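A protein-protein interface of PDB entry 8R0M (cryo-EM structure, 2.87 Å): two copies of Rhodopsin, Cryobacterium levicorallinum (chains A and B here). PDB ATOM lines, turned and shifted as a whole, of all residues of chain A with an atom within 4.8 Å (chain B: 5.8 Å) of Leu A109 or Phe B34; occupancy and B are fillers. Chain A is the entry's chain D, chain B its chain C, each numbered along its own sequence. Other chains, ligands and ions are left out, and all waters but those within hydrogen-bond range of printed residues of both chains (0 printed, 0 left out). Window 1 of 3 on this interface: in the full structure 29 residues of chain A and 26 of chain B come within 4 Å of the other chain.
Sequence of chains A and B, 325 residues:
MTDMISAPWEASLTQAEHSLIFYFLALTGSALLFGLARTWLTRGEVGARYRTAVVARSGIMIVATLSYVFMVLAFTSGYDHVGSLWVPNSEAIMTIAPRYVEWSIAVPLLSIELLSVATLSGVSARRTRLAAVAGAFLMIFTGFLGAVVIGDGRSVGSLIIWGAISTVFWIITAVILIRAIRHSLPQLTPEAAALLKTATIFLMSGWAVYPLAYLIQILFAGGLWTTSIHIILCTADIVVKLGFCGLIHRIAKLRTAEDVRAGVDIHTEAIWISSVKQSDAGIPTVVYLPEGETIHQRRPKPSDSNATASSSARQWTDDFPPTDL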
ATOM      1  N   VAL A  55      20.865  24.347   7.910  1.00  0.00           N
ATOM      2  CA  VAL A  55      20.952  23.347   6.871  1.00  0.00           C
ATOM      3  C   VAL A  55      22.268  23.564   6.139  1.00  0.00           C
ATOM      4  O   VAL A  55      23.045  22.621   5.992  1.00  0.00           O
ATOM      5  CB  VAL A  55      19.716  23.471   5.953  1.00  0.00           C
ATOM      6  CG1 VAL A  55      19.873  22.812   4.588  1.00  0.00           C
ATOM      7  CG2 VAL A  55      18.488  22.912   6.654  1.00  0.00           C
ATOM      8  N   ALA A  56      22.514  24.807   5.715  1.00  0.00           N
ATOM      9  CA  ALA A  56      23.787  25.152   5.121  1.00  0.00           C
ATOM     10  C   ALA A  56      24.930  24.601   5.978  1.00  0.00           C
ATOM     11  O   ALA A  56      25.621  23.668   5.563  1.00  0.00           O
ATOM     12  CB  ALA A  56      23.879  26.641   4.948  1.00  0.00           C
ATOM     13  N   GLY A  59      25.611  20.976   5.978  1.00  0.00           N
ATOM     14  CA  GLY A  59      26.208  20.498   4.747  1.00  0.00           C
ATOM     15  C   GLY A  59      27.691  20.800   4.768  1.00  0.00           C
ATOM     16  O   GLY A  59      28.520  19.920   4.587  1.00  0.00           O
ATOM     17  N   ILE A  60      28.013  22.032   5.125  1.00  0.00           N
ATOM     18  CA  ILE A  60      29.396  22.440   5.177  1.00  0.00           C
ATOM     19  C   ILE A  60      30.190  21.491   6.065  1.00  0.00           C
ATOM     20  O   ILE A  60      31.320  21.169   5.730  1.00  0.00           O
ATOM     21  CB  ILE A  60      29.508  23.900   5.614  1.00  0.00           C
ATOM     22  CG1 ILE A  60      28.750  24.778   4.624  1.00  0.00           C
ATOM     23  CG2 ILE A  60      30.954  24.321   5.732  1.00  0.00           C
ATOM     24  CD1 ILE A  60      28.627  26.229   5.045  1.00  0.00           C
ATOM     25  N   ILE A 105      31.154  22.209  -2.777  1.00  0.00           N
ATOM     26  CA  ILE A 105      29.874  22.252  -2.099  1.00  0.00           C
ATOM     27  C   ILE A 105      29.878  23.420  -1.115  1.00  0.00           C
ATOM     28  O   ILE A 105      29.022  24.291  -1.199  1.00  0.00           O
ATOM     29  CB  ILE A 105      29.582  20.911  -1.406  1.00  0.00           C
ATOM     30  CG1 ILE A 105      29.735  19.710  -2.342  1.00  0.00           C
ATOM     31  CG2 ILE A 105      28.217  20.924  -0.768  1.00  0.00           C
ATOM     32  CD1 ILE A 105      28.771  19.715  -3.499  1.00  0.00           C
ATOM     33  N   ALA A 106      30.881  23.470  -0.239  1.00  0.00           N
ATOM     34  CA  ALA A 106      30.975  24.445   0.837  1.00  0.00           C
ATOM     35  C   ALA A 106      31.025  25.880   0.345  1.00  0.00           C
ATOM     36  O   ALA A 106      30.346  26.716   0.899  1.00  0.00           O
ATOM     37  CB  ALA A 106      32.166  24.170   1.707  1.00  0.00           C
ATOM     38  N   VAL A 107      31.827  26.242  -0.617  1.00  0.00           N
ATOM     39  CA  VAL A 107      31.888  27.671  -0.859  1.00  0.00           C
ATOM     40  C   VAL A 107      30.516  28.192  -1.273  1.00  0.00           C
ATOM     41  O   VAL A 107      30.131  29.287  -0.876  1.00  0.00           O
ATOM     42  CB  VAL A 107      32.999  28.044  -1.848  1.00  0.00           C
ATOM     43  CG1 VAL A 107      32.981  29.518  -2.221  1.00  0.00           C
ATOM     44  CG2 VAL A 107      34.328  27.643  -1.224  1.00  0.00           C
ATOM     45  N   PRO A 108      29.754  27.479  -2.122  1.00  0.00           N
ATOM     46  CA  PRO A 108      28.369  27.839  -2.411  1.00  0.00           C
ATOM     47  C   PRO A 108      27.471  27.863  -1.169  1.00  0.00           C
ATOM     48  O   PRO A 108      26.725  28.819  -0.984  1.00  0.00           O
ATOM     49  CB  PRO A 108      27.978  26.718  -3.370  1.00  0.00           C
ATOM     50  CG  PRO A 108      29.229  26.491  -4.112  1.00  0.00           C
ATOM     51  CD  PRO A 108      30.228  26.400  -2.984  1.00  0.00           C
ATOM     52  N   LEU A 109      27.550  26.829  -0.317  1.00  0.00           N
ATOM     53  CA  LEU A 109      26.783  26.785   0.917  1.00  0.00           C
ATOM     54  C   LEU A 109      27.208  27.878   1.885  1.00  0.00           C
ATOM     55  O   LEU A 109      26.387  28.320   2.652  1.00  0.00           O
ATOM     56  CB  LEU A 109      26.916  25.428   1.613  1.00  0.00           C
ATOM     57  CG  LEU A 109      26.142  24.277   0.973  1.00  0.00           C
ATOM     58  CD1 LEU A 109      26.203  23.018   1.836  1.00  0.00           C
ATOM     59  CD2 LEU A 109      24.677  24.650   0.709  1.00  0.00           C
ATOM     60  N   LEU A 110      28.460  28.318   1.922  1.00  0.00           N
ATOM     61  CA  LEU A 110      28.800  29.400   2.832  1.00  0.00           C
ATOM     62  C   LEU A 110      28.090  30.646   2.350  1.00  0.00           C
ATOM     63  O   LEU A 110      27.746  31.490   3.149  1.00  0.00           O
ATOM     64  CB  LEU A 110      30.319  29.630   2.908  1.00  0.00           C
ATOM     65  CG  LEU A 110      31.086  28.593   3.742  1.00  0.00           C
ATOM     66  CD1 LEU A 110      32.558  28.540   3.383  1.00  0.00           C
ATOM     67  CD2 LEU A 110      30.950  28.886   5.225  1.00  0.00           C
ATOM     68  N   SER A 111      27.907  30.771   1.043  1.00  0.00           N
ATOM     69  CA  SER A 111      27.316  31.970   0.494  1.00  0.00           C
ATOM     70  C   SER A 111      25.849  31.970   0.846  1.00  0.00           C
ATOM     71  O   SER A 111      25.298  33.030   1.097  1.00  0.00           O
ATOM     72  CB  SER A 111      27.487  32.045  -0.986  1.00  0.00           C
ATOM     73  OG  SER A 111      28.817  31.717  -1.365  1.00  0.00           O
ATOM     74  N   ILE A 112      25.245  30.773   0.820  1.00  0.00           N
ATOM     75  CA  ILE A 112      23.835  30.588   1.119  1.00  0.00           C
ATOM     76  C   ILE A 112      23.586  30.869   2.591  1.00  0.00           C
ATOM     77  O   ILE A 112      22.635  31.568   2.916  1.00  0.00           O
ATOM     78  CB  ILE A 112      23.398  29.177   0.709  1.00  0.00           C
ATOM     79  CG1 ILE A 112      23.050  29.171  -0.774  1.00  0.00           C
ATOM     80  CG2 ILE A 112      22.255  28.621   1.541  1.00  0.00           C
ATOM     81  CD1 ILE A 112      22.801  27.773  -1.281  1.00  0.00           C
ATOM     82  N   GLU A 113      24.444  30.346   3.458  1.00  0.00           N
ATOM     83  CA  GLU A 113      24.360  30.613   4.881  1.00  0.00           C
ATOM     84  C   GLU A 113      24.433  32.109   5.164  1.00  0.00           C
ATOM     85  O   GLU A 113      23.720  32.609   6.019  1.00  0.00           O
ATOM     86  CB  GLU A 113      25.482  29.923   5.642  1.00  0.00           C
ATOM     87  CG  GLU A 113      25.194  29.772   7.107  1.00  0.00           C
ATOM     88  CD  GLU A 113      26.239  28.950   7.850  1.00  0.00           C
ATOM     89  OE1 GLU A 113      25.991  28.590   9.056  1.00  0.00           O
ATOM     90  OE2 GLU A 113      27.321  28.686   7.234  1.00  0.00           O
ATOM     91  N   GLY B  29      28.313  12.251  -4.508  1.00  0.00           N
ATOM     92  CA  GLY B  29      28.058  11.658  -3.191  1.00  0.00           C
ATOM     93  C   GLY B  29      28.024  12.692  -2.099  1.00  0.00           C
ATOM     94  O   GLY B  29      27.383  12.419  -1.107  1.00  0.00           O
ATOM     95  N   SER B  30      28.791  13.767  -2.227  1.00  0.00           N
ATOM     96  CA  SER B  30      28.861  14.880  -1.263  1.00  0.00           C
ATOM     97  C   SER B  30      27.570  15.674  -1.276  1.00  0.00           C
ATOM     98  O   SER B  30      27.127  16.029  -0.201  1.00  0.00           O
ATOM     99  CB  SER B  30      29.997  15.747  -1.652  1.00  0.00           C
ATOM    100  OG  SER B  30      31.205  15.015  -1.635  1.00  0.00           O
ATOM    101  N   ALA B  31      27.015  15.949  -2.442  1.00  0.00           N
ATOM    102  CA  ALA B  31      25.779  16.735  -2.597  1.00  0.00           C
ATOM    103  C   ALA B  31      24.547  15.937  -2.198  1.00  0.00           C
ATOM    104  O   ALA B  31      23.539  16.539  -1.892  1.00  0.00           O
ATOM    105  CB  ALA B  31      25.688  17.165  -4.005  1.00  0.00           C
ATOM    106  N   LEU B  32      24.631  14.626  -2.217  1.00  0.00           N
ATOM    107  CA  LEU B  32      23.478  13.765  -1.896  1.00  0.00           C
ATOM    108  C   LEU B  32      23.585  13.369  -0.438  1.00  0.00           C
ATOM    109  O   LEU B  32      22.661  12.752   0.050  1.00  0.00           O
ATOM    110  CB  LEU B  32      23.500  12.571  -2.848  1.00  0.00           C
ATOM    111  CG  LEU B  32      23.333  12.881  -4.334  1.00  0.00           C
ATOM    112  CD1 LEU B  32      23.390  11.608  -5.158  1.00  0.00           C
ATOM    113  CD2 LEU B  32      22.041  13.629  -4.611  1.00  0.00           C
ATOM    114  N   LEU B  33      24.640  13.774   0.251  1.00  0.00           N
ATOM    115  CA  LEU B  33      24.751  13.576   1.719  1.00  0.00           C
ATOM    116  C   LEU B  33      24.315  14.892   2.346  1.00  0.00           C
ATOM    117  O   LEU B  33      23.910  14.866   3.493  1.00  0.00           O
ATOM    118  CB  LEU B  33      26.172  13.164   2.092  1.00  0.00           C
ATOM    119  CG  LEU B  33      26.390  12.674   3.520  1.00  0.00           C
ATOM    120  CD1 LEU B  33      25.481  11.505   3.845  1.00  0.00           C
ATOM    121  CD2 LEU B  33      27.837  12.277   3.717  1.00  0.00           C
ATOM    122  N   PHE B  34      24.441  16.008   1.642  1.00  0.00           N
ATOM    123  CA  PHE B  34      23.860  17.291   2.071  1.00  0.00           C
ATOM    124  C   PHE B  34      22.342  17.193   1.941  1.00  0.00           C
ATOM    125  O   PHE B  34      21.654  17.733   2.794  1.00  0.00           O
ATOM    126  CB  PHE B  34      24.350  18.419   1.174  1.00  0.00           C
ATOM    127  CG  PHE B  34      23.541  19.687   1.228  1.00  0.00           C
ATOM    128  CD1 PHE B  34      23.346  20.357   2.421  1.00  0.00           C
ATOM    129  CD2 PHE B  34      22.979  20.212   0.081  1.00  0.00           C
ATOM    130  CE1 PHE B  34      22.596  21.518   2.466  1.00  0.00           C
ATOM    131  CE2 PHE B  34      22.227  21.370   0.128  1.00  0.00           C
ATOM    132  CZ  PHE B  34      22.042  22.025   1.320  1.00  0.00           C
ATOM    133  N   GLY B  35      21.829  16.574   0.895  1.00  0.00           N
ATOM    134  CA  GLY B  35      20.400  16.415   0.715  1.00  0.00           C
ATOM    135  C   GLY B  35      19.831  15.475   1.734  1.00  0.00           C
ATOM    136  O   GLY B  35      18.661  15.614   2.011  1.00  0.00           O
ATOM    137  N   LEU B  36      20.587  14.488   2.189  1.00  0.00           N
ATOM    138  CA  LEU B  36      20.115  13.578   3.263  1.00  0.00           C
ATOM    139  C   LEU B  36      20.012  14.348   4.571  1.00  0.00           C
ATOM    140  O   LEU B  36      19.067  14.130   5.288  1.00  0.00           O
ATOM    141  CB  LEU B  36      21.068  12.387   3.378  1.00  0.00           C
ATOM    142  CG  LEU B  36      20.597  11.237   4.260  1.00  0.00           C
ATOM    143  CD1 LEU B  36      19.227  10.748   3.823  1.00  0.00           C
ATOM    144  CD2 LEU B  36      21.613  10.112   4.227  1.00  0.00           C
ATOM    145  N   ALA B  37      20.975  15.183   4.873  1.00  0.00           N
ATOM    146  CA  ALA B  37      20.957  16.038   6.061  1.00  0.00           C
ATOM    147  C   ALA B  37      19.842  17.066   5.965  1.00  0.00           C
ATOM    148  O   ALA B  37      19.191  17.240   6.955  1.00  0.00           O
ATOM    149  CB  ALA B  37      22.275  16.734   6.091  1.00  0.00           C
ATOM    150  N   ARG B  38      19.655  17.736   4.834  1.00  0.00           N
ATOM    151  CA  ARG B  38      18.620  18.762   4.630  1.00  0.00           C
ATOM    152  C   ARG B  38      17.292  18.081   4.842  1.00  0.00           C
ATOM    153  O   ARG B  38      16.459  18.683   5.441  1.00  0.00           O
ATOM    154  CB  ARG B  38      18.727  19.245   3.188  1.00  0.00           C
ATOM    155  CG  ARG B  38      17.763  20.334   2.765  1.00  0.00           C
ATOM    156  CD  ARG B  38      18.367  20.857   1.486  1.00  0.00           C
ATOM    157  NE  ARG B  38      17.494  21.736   0.732  1.00  0.00           N
ATOM    158  CZ  ARG B  38      17.236  21.599  -0.561  1.00  0.00           C
ATOM    159  NH1 ARG B  38      17.836  20.655  -1.261  1.00  0.00           N
ATOM    160  NH2 ARG B  38      16.383  22.418  -1.150  1.00  0.00           N
ATOM    161  N   THR B  39      17.110  16.866   4.370  1.00  0.00           N
ATOM    162  CA  THR B  39      15.832  16.123   4.419  1.00  0.00           C
ATOM    163  C   THR B  39      15.435  15.850   5.858  1.00  0.00           C
ATOM    164  O   THR B  39      14.250  15.918   6.116  1.00  0.00           O
ATOM    165  CB  THR B  39      15.957  14.840   3.585  1.00  0.00           C
ATOM    166  OG1 THR B  39      16.263  15.217   2.247  1.00  0.00           O
ATOM    167  CG2 THR B  39      14.702  14.003   3.595  1.00  0.00           C
ATOM    168  N   LEU B 242      18.723  16.882  -5.980  1.00  0.00           N
ATOM    169  CA  LEU B 242      18.642  18.072  -5.153  1.00  0.00           C
ATOM    170  C   LEU B 242      17.484  18.941  -5.625  1.00  0.00           C
ATOM    171  O   LEU B 242      16.536  19.151  -4.871  1.00  0.00           O
ATOM    172  CB  LEU B 242      19.965  18.824  -5.172  1.00  0.00           C
ATOM    173  CG  LEU B 242      21.070  18.182  -4.334  1.00  0.00           C
ATOM    174  CD1 LEU B 242      22.227  19.153  -4.152  1.00  0.00           C
ATOM    175  CD2 LEU B 242      20.576  17.720  -2.969  1.00  0.00           C
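Of the 13 printed residues of chain A, 3 touch a printed residue of chain B. Of the 12 printed residues of chain B, 2 touch a printed residue of chain A. Hydrophobic or aromatic side chains of chain B within 4 Å of the printed part of chain A: Phe B34.
Phe B34 touches Val A55 (CE1 to CG1, 3.7 Å). Arg B38 touches Val A55 (CG to CG1, 3.7 Å). Phe B34 touches Gly A59. CZ of Phe B34 touches CD2 of Leu A109 (3.8 Å).
No position is printed for both chains. Of the 4 pairs that touch across the chains among the printed residues, none has its exchanged pair printed and touching as well.
Leu A109 touches one residue of chain B. Phe B34 touches just these residues of chain A: Val A55, Gly A59 and Leu A109. Of the printed residues of chain B, Val A55 touches Phe B34 and Arg B38. Of the printed residues of chain B, Gly A59 touches Phe B34. Of the printed residues of chain A, Arg B38 touches Val A55 (3.7 Å). The nearest printed residue of chain B that does not touch Leu A109 is Ser B30 (7.3 Å).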
